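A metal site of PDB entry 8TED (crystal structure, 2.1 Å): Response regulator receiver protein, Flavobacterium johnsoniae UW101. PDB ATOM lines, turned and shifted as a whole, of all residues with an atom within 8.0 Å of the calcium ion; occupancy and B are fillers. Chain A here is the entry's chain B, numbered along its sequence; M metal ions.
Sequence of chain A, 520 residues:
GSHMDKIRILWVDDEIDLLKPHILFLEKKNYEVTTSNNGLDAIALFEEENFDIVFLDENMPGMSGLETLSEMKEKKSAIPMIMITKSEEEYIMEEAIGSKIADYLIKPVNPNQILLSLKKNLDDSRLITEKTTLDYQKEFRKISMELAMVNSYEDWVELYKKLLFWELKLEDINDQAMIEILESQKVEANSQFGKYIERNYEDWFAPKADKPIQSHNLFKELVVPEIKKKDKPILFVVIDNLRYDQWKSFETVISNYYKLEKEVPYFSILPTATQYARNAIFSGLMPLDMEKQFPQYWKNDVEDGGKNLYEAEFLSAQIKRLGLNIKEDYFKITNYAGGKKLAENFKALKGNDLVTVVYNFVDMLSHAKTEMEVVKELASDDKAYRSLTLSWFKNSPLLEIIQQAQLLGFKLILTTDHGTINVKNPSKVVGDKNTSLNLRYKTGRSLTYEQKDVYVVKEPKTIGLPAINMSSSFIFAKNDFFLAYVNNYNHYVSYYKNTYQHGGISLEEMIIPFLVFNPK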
ATOM      1  N   VAL A 238       6.556   2.686  20.590  1.00  0.00           N
ATOM      2  CA  VAL A 238       6.593   2.570  19.104  1.00  0.00           C
ATOM      3  C   VAL A 238       8.055   2.458  18.684  1.00  0.00           C
ATOM      4  O   VAL A 238       8.793   3.446  18.802  1.00  0.00           O
ATOM      5  CB  VAL A 238       5.867   3.743  18.418  1.00  0.00           C
ATOM      6  CG1 VAL A 238       5.753   3.483  16.922  1.00  0.00           C
ATOM      7  CG2 VAL A 238       4.502   3.963  19.032  1.00  0.00           C
ATOM      8  N   ILE A 239       8.472   1.272  18.275  1.00  0.00           N
ATOM      9  CA  ILE A 239       9.797   1.095  17.601  1.00  0.00           C
ATOM     10  C   ILE A 239       9.639   1.539  16.154  1.00  0.00           C
ATOM     11  O   ILE A 239       8.897   0.897  15.413  1.00  0.00           O
ATOM     12  CB  ILE A 239      10.325  -0.347  17.690  1.00  0.00           C
ATOM     13  CG1 ILE A 239      10.455  -0.768  19.146  1.00  0.00           C
ATOM     14  CG2 ILE A 239      11.656  -0.445  16.969  1.00  0.00           C
ATOM     15  CD1 ILE A 239      10.839  -2.211  19.343  1.00  0.00           C
ATOM     16  N   ASP A 240      10.365   2.600  15.787  1.00  0.00           N
ATOM     17  CA  ASP A 240      10.383   3.137  14.395  1.00  0.00           C
ATOM     18  C   ASP A 240      10.788   2.029  13.401  1.00  0.00           C
ATOM     19  O   ASP A 240      11.771   1.364  13.645  1.00  0.00           O
ATOM     20  CB  ASP A 240      11.369   4.312  14.333  1.00  0.00           C
ATOM     21  CG  ASP A 240      11.175   5.144  13.092  1.00  0.00           C
ATOM     22  OD1 ASP A 240      10.022   5.562  12.845  1.00  0.00           O
ATOM     23  OD2 ASP A 240      12.202   5.417  12.435  1.00  0.00           O
ATOM     24  N   ASN A 241      10.020   1.835  12.348  1.00  0.00           N
ATOM     25  CA  ASN A 241      10.422   1.116  11.117  1.00  0.00           C
ATOM     26  C   ASN A 241      10.498  -0.395  11.372  1.00  0.00           C
ATOM     27  O   ASN A 241      11.155  -1.003  10.594  1.00  0.00           O
ATOM     28  CB  ASN A 241      11.786   1.580  10.586  1.00  0.00           C
ATOM     29  CG  ASN A 241      11.792   2.980  10.007  1.00  0.00           C
ATOM     30  OD1 ASN A 241      10.816   3.722  10.102  1.00  0.00           O
ATOM     31  ND2 ASN A 241      12.898   3.358   9.395  1.00  0.00           N
ATOM     32  N   LEU A 242       9.801  -0.973  12.363  1.00  0.00           N
ATOM     33  CA  LEU A 242       9.969  -2.406  12.734  1.00  0.00           C
ATOM     34  C   LEU A 242       9.090  -3.310  11.867  1.00  0.00           C
ATOM     35  O   LEU A 242       7.879  -3.030  11.768  1.00  0.00           O
ATOM     36  CB  LEU A 242       9.634  -2.607  14.216  1.00  0.00           C
ATOM     37  CG  LEU A 242      10.024  -3.986  14.748  1.00  0.00           C
ATOM     38  CD1 LEU A 242      11.526  -4.053  14.963  1.00  0.00           C
ATOM     39  CD2 LEU A 242       9.309  -4.342  16.036  1.00  0.00           C
ATOM     40  N   THR A 272       3.696   4.311   3.688  1.00  0.00           N
ATOM     41  CA  THR A 272       4.297   3.558   4.820  1.00  0.00           C
ATOM     42  C   THR A 272       5.551   4.300   5.260  1.00  0.00           C
ATOM     43  O   THR A 272       6.673   3.769   5.065  1.00  0.00           O
ATOM     44  CB  THR A 272       4.525   2.102   4.414  1.00  0.00           C
ATOM     45  OG1 THR A 272       5.173   2.082   3.151  1.00  0.00           O
ATOM     46  CG2 THR A 272       3.226   1.344   4.348  1.00  0.00           C
ATOM     47  N   ALA A 273       5.389   5.482   5.840  1.00  0.00           N
ATOM     48  CA  ALA A 273       6.497   6.402   6.187  1.00  0.00           C
ATOM     49  C   ALA A 273       6.100   7.198   7.432  1.00  0.00           C
ATOM     50  O   ALA A 273       4.911   7.583   7.590  1.00  0.00           O
ATOM     51  CB  ALA A 273       6.816   7.332   5.032  1.00  0.00           C
ATOM     52  N   THR A 274       7.103   7.421   8.270  1.00  0.00           N
ATOM     53  CA  THR A 274       7.025   8.019   9.622  1.00  0.00           C
ATOM     54  C   THR A 274       6.160   9.274   9.633  1.00  0.00           C
ATOM     55  O   THR A 274       5.305   9.379  10.518  1.00  0.00           O
ATOM     56  CB  THR A 274       8.439   8.343  10.108  1.00  0.00           C
ATOM     57  OG1 THR A 274       9.280   7.255   9.705  1.00  0.00           O
ATOM     58  CG2 THR A 274       8.508   8.544  11.593  1.00  0.00           C
ATOM     59  N   GLN A 275       6.407  10.208   8.704  1.00  0.00           N
ATOM     60  CA  GLN A 275       5.756  11.539   8.661  1.00  0.00           C
ATOM     61  C   GLN A 275       4.223  11.396   8.579  1.00  0.00           C
ATOM     62  O   GLN A 275       3.494  12.241   9.134  1.00  0.00           O
ATOM     63  CB  GLN A 275       6.319  12.314   7.480  1.00  0.00           C
ATOM     64  CG  GLN A 275       5.555  13.591   7.156  1.00  0.00           C
ATOM     65  CD  GLN A 275       6.049  14.195   5.867  1.00  0.00           C
ATOM     66  OE1 GLN A 275       7.040  13.755   5.302  1.00  0.00           O
ATOM     67  NE2 GLN A 275       5.411  15.267   5.417  1.00  0.00           N
ATOM     68  N   TYR A 276       3.762  10.352   7.896  1.00  0.00           N
ATOM     69  CA  TYR A 276       2.302  10.075   7.687  1.00  0.00           C
ATOM     70  C   TYR A 276       1.811   9.071   8.737  1.00  0.00           C
ATOM     71  O   TYR A 276       0.919   9.453   9.509  1.00  0.00           O
ATOM     72  CB  TYR A 276       2.100   9.645   6.246  1.00  0.00           C
ATOM     73  CG  TYR A 276       2.509  10.690   5.235  1.00  0.00           C
ATOM     74  CD1 TYR A 276       1.578  11.563   4.697  1.00  0.00           C
ATOM     75  CD2 TYR A 276       3.828  10.830   4.860  1.00  0.00           C
ATOM     76  CE1 TYR A 276       1.951  12.550   3.803  1.00  0.00           C
ATOM     77  CE2 TYR A 276       4.220  11.825   3.956  1.00  0.00           C
ATOM     78  CZ  TYR A 276       3.267  12.671   3.417  1.00  0.00           C
ATOM     79  OH  TYR A 276       3.630  13.616   2.491  1.00  0.00           O
ATOM     80  N   ALA A 277       2.368   7.852   8.783  1.00  0.00           N
ATOM     81  CA  ALA A 277       1.851   6.717   9.593  1.00  0.00           C
ATOM     82  C   ALA A 277       2.038   7.001  11.088  1.00  0.00           C
ATOM     83  O   ALA A 277       1.096   6.788  11.874  1.00  0.00           O
ATOM     84  CB  ALA A 277       2.518   5.427   9.210  1.00  0.00           C
ATOM     85  N   ARG A 278       3.213   7.511  11.484  1.00  0.00           N
ATOM     86  CA  ARG A 278       3.548   7.637  12.914  1.00  0.00           C
ATOM     87  C   ARG A 278       2.784   8.840  13.488  1.00  0.00           C
ATOM     88  O   ARG A 278       2.251   8.708  14.622  1.00  0.00           O
ATOM     89  CB  ARG A 278       5.058   7.732  13.152  1.00  0.00           C
ATOM     90  CG  ARG A 278       5.427   7.148  14.504  1.00  0.00           C
ATOM     91  CD  ARG A 278       6.915   7.016  14.774  1.00  0.00           C
ATOM     92  NE  ARG A 278       7.482   8.309  15.071  1.00  0.00           N
ATOM     93  CZ  ARG A 278       8.777   8.594  15.065  1.00  0.00           C
ATOM     94  NH1 ARG A 278       9.670   7.683  14.722  1.00  0.00           N
ATOM     95  NH2 ARG A 278       9.157   9.798  15.404  1.00  0.00           N
ATOM     96  N   ASN A 308       8.367  14.891  12.354  1.00  0.00           N
ATOM     97  CA  ASN A 308       7.702  14.235  13.512  1.00  0.00           C
ATOM     98  C   ASN A 308       8.060  14.982  14.812  1.00  0.00           C
ATOM     99  O   ASN A 308       8.192  14.324  15.863  1.00  0.00           O
ATOM    100  CB  ASN A 308       7.988  12.736  13.570  1.00  0.00           C
ATOM    101  CG  ASN A 308       7.314  11.967  12.460  1.00  0.00           C
ATOM    102  OD1 ASN A 308       6.212  11.419  12.640  1.00  0.00           O
ATOM    103  ND2 ASN A 308       7.931  11.960  11.296  1.00  0.00           N
ATOM    104  N   GLU A 311       4.616  15.024  17.943  1.00  0.00           N
ATOM    105  CA  GLU A 311       3.874  13.797  18.327  1.00  0.00           C
ATOM    106  C   GLU A 311       3.311  13.928  19.751  1.00  0.00           C
ATOM    107  O   GLU A 311       2.168  13.470  19.964  1.00  0.00           O
ATOM    108  CB  GLU A 311       4.767  12.563  18.149  1.00  0.00           C
ATOM    109  CG  GLU A 311       5.090  12.277  16.703  1.00  0.00           C
ATOM    110  CD  GLU A 311       5.981  11.078  16.421  1.00  0.00           C
ATOM    111  OE1 GLU A 311       6.795  10.719  17.300  1.00  0.00           O
ATOM    112  OE2 GLU A 311       5.820  10.498  15.331  1.00  0.00           O
ATOM    113  N   VAL A 358       8.795   6.610  21.675  1.00  0.00           N
ATOM    114  CA  VAL A 358       9.257   6.351  20.300  1.00  0.00           C
ATOM    115  C   VAL A 358      10.743   6.000  20.373  1.00  0.00           C
ATOM    116  O   VAL A 358      11.503   6.819  20.944  1.00  0.00           O
ATOM    117  CB  VAL A 358       9.037   7.588  19.422  1.00  0.00           C
ATOM    118  CG1 VAL A 358       9.646   7.374  18.043  1.00  0.00           C
ATOM    119  CG2 VAL A 358       7.553   7.924  19.321  1.00  0.00           C
ATOM    120  N   ASN A 360      13.884   4.952  17.967  1.00  0.00           N
ATOM    121  CA  ASN A 360      14.374   4.863  16.580  1.00  0.00           C
ATOM    122  C   ASN A 360      15.331   3.678  16.497  1.00  0.00           C
ATOM    123  O   ASN A 360      16.030   3.385  17.472  1.00  0.00           O
ATOM    124  CB  ASN A 360      14.966   6.191  16.090  1.00  0.00           C
ATOM    125  CG  ASN A 360      13.929   7.263  15.832  1.00  0.00           C
ATOM    126  OD1 ASN A 360      12.727   7.035  15.894  1.00  0.00           O
ATOM    127  ND2 ASN A 360      14.381   8.464  15.558  1.00  0.00           N
ATOM    128  N   THR A 416       4.720  -0.510  16.079  1.00  0.00           N
ATOM    129  CA  THR A 416       5.561   0.176  15.074  1.00  0.00           C
ATOM    130  C   THR A 416       4.634   0.958  14.166  1.00  0.00           C
ATOM    131  O   THR A 416       3.413   0.730  14.234  1.00  0.00           O
ATOM    132  CB  THR A 416       6.407  -0.825  14.270  1.00  0.00           C
ATOM    133  OG1 THR A 416       7.263  -0.075  13.403  1.00  0.00           O
ATOM    134  CG2 THR A 416       5.559  -1.793  13.466  1.00  0.00           C
ATOM    135  N   ASP A 417       5.210   1.805  13.312  1.00  0.00           N
ATOM    136  CA  ASP A 417       4.430   2.640  12.372  1.00  0.00           C
ATOM    137  C   ASP A 417       4.356   1.973  11.003  1.00  0.00           C
ATOM    138  O   ASP A 417       3.321   2.146  10.318  1.00  0.00           O
ATOM    139  CB  ASP A 417       4.996   4.059  12.343  1.00  0.00           C
ATOM    140  CG  ASP A 417       6.477   4.157  12.011  1.00  0.00           C
ATOM    141  OD1 ASP A 417       7.219   3.148  12.137  1.00  0.00           O
ATOM    142  OD2 ASP A 417       6.877   5.270  11.674  1.00  0.00           O
ATOM    143  N   HIS A 418       5.413   1.259  10.611  1.00  0.00           N
ATOM    144  CA  HIS A 418       5.513   0.539   9.324  1.00  0.00           C
ATOM    145  C   HIS A 418       6.796  -0.273   9.301  1.00  0.00           C
ATOM    146  O   HIS A 418       7.720  -0.016  10.121  1.00  0.00           O
ATOM    147  CB  HIS A 418       5.434   1.514   8.142  1.00  0.00           C
ATOM    148  CG  HIS A 418       6.571   2.478   8.130  1.00  0.00           C
ATOM    149  ND1 HIS A 418       7.813   2.121   7.685  1.00  0.00           N
ATOM    150  CD2 HIS A 418       6.687   3.730   8.625  1.00  0.00           C
ATOM    151  CE1 HIS A 418       8.642   3.135   7.890  1.00  0.00           C
ATOM    152  NE2 HIS A 418       7.972   4.125   8.462  1.00  0.00           N
ATOM    153  N   GLY A 419       6.875  -1.220   8.370  1.00  0.00           N
ATOM    154  CA  GLY A 419       8.101  -2.010   8.172  1.00  0.00           C
ATOM    155  C   GLY A 419       8.946  -1.440   7.052  1.00  0.00           C
ATOM    156  O   GLY A 419       8.776  -0.265   6.712  1.00  0.00           O
ATOM    157  N   THR A 420       9.863  -2.267   6.556  1.00  0.00           N
ATOM    158  CA  THR A 420      10.797  -1.947   5.457  1.00  0.00           C
ATOM    159  C   THR A 420      10.956  -3.195   4.579  1.00  0.00           C
ATOM    160  O   THR A 420      10.640  -4.307   5.044  1.00  0.00           O
ATOM    161  CB  THR A 420      12.170  -1.471   5.940  1.00  0.00           C
ATOM    162  OG1 THR A 420      12.781  -2.609   6.535  1.00  0.00           O
ATOM    163  CG2 THR A 420      12.175  -0.289   6.899  1.00  0.00           C
ATOM    164  N   HIS A 502      11.143   1.967   2.646  1.00  0.00           N
ATOM    165  CA  HIS A 502       9.737   2.035   3.073  1.00  0.00           C
ATOM    166  C   HIS A 502       9.056   3.175   2.332  1.00  0.00           C
ATOM    167  O   HIS A 502       9.773   4.039   1.746  1.00  0.00           O
ATOM    168  CB  HIS A 502       9.652   2.166   4.603  1.00  0.00           C
ATOM    169  CG  HIS A 502      10.330   3.384   5.112  1.00  0.00           C
ATOM    170  ND1 HIS A 502       9.665   4.601   5.249  1.00  0.00           N
ATOM    171  CD2 HIS A 502      11.611   3.596   5.515  1.00  0.00           C
ATOM    172  CE1 HIS A 502      10.504   5.493   5.738  1.00  0.00           C
ATOM    173  NE2 HIS A 502      11.705   4.901   5.878  1.00  0.00           N
HETATM  174 CA    CA M   1       9.026   5.086  10.659  1.00  0.00          CA
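The calcium ion is bound by OD1 of Asn 241 (2.3 Å), OG1 of Thr 274 (2.4 Å), OD2 of Asp 417 (2.4 Å), OD1 of Asp 240 (2.4 Å) and NE2 of His 418 (2.6 Å). Slightly farther from the calcium ion lies OD1 of Asp 417 (3.0 Å).
A ring nitrogen (ND1) of His 418 is in hydrogen-bond range of the backbone carbonyl oxygen (O) of Thr 272 (3.3 Å). The side-chain hydroxyl (OG1) of Thr 416 lies within hydrogen-bond range of the side-chain carboxylate (OD1) of Asp 417 (3.5 Å). The backbone carbonyl oxygen (O) of Thr 274 sits close to the side-chain amide oxygen (OD1) of Asn 308. O of His 418 sits at hydrogen-bond distance from OG1 of Thr 416, at 3.3 Å. NH1 of Arg 278 sits close to OD1 of Asp 240 (2.9 Å). The backbone carbonyl oxygen of His 418 is in hydrogen-bond range of the backbone NH of Leu 242 (3.2 Å).
The nearest printed residue that does not touch the calcium ion is Ala 273 (4.8 Å).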
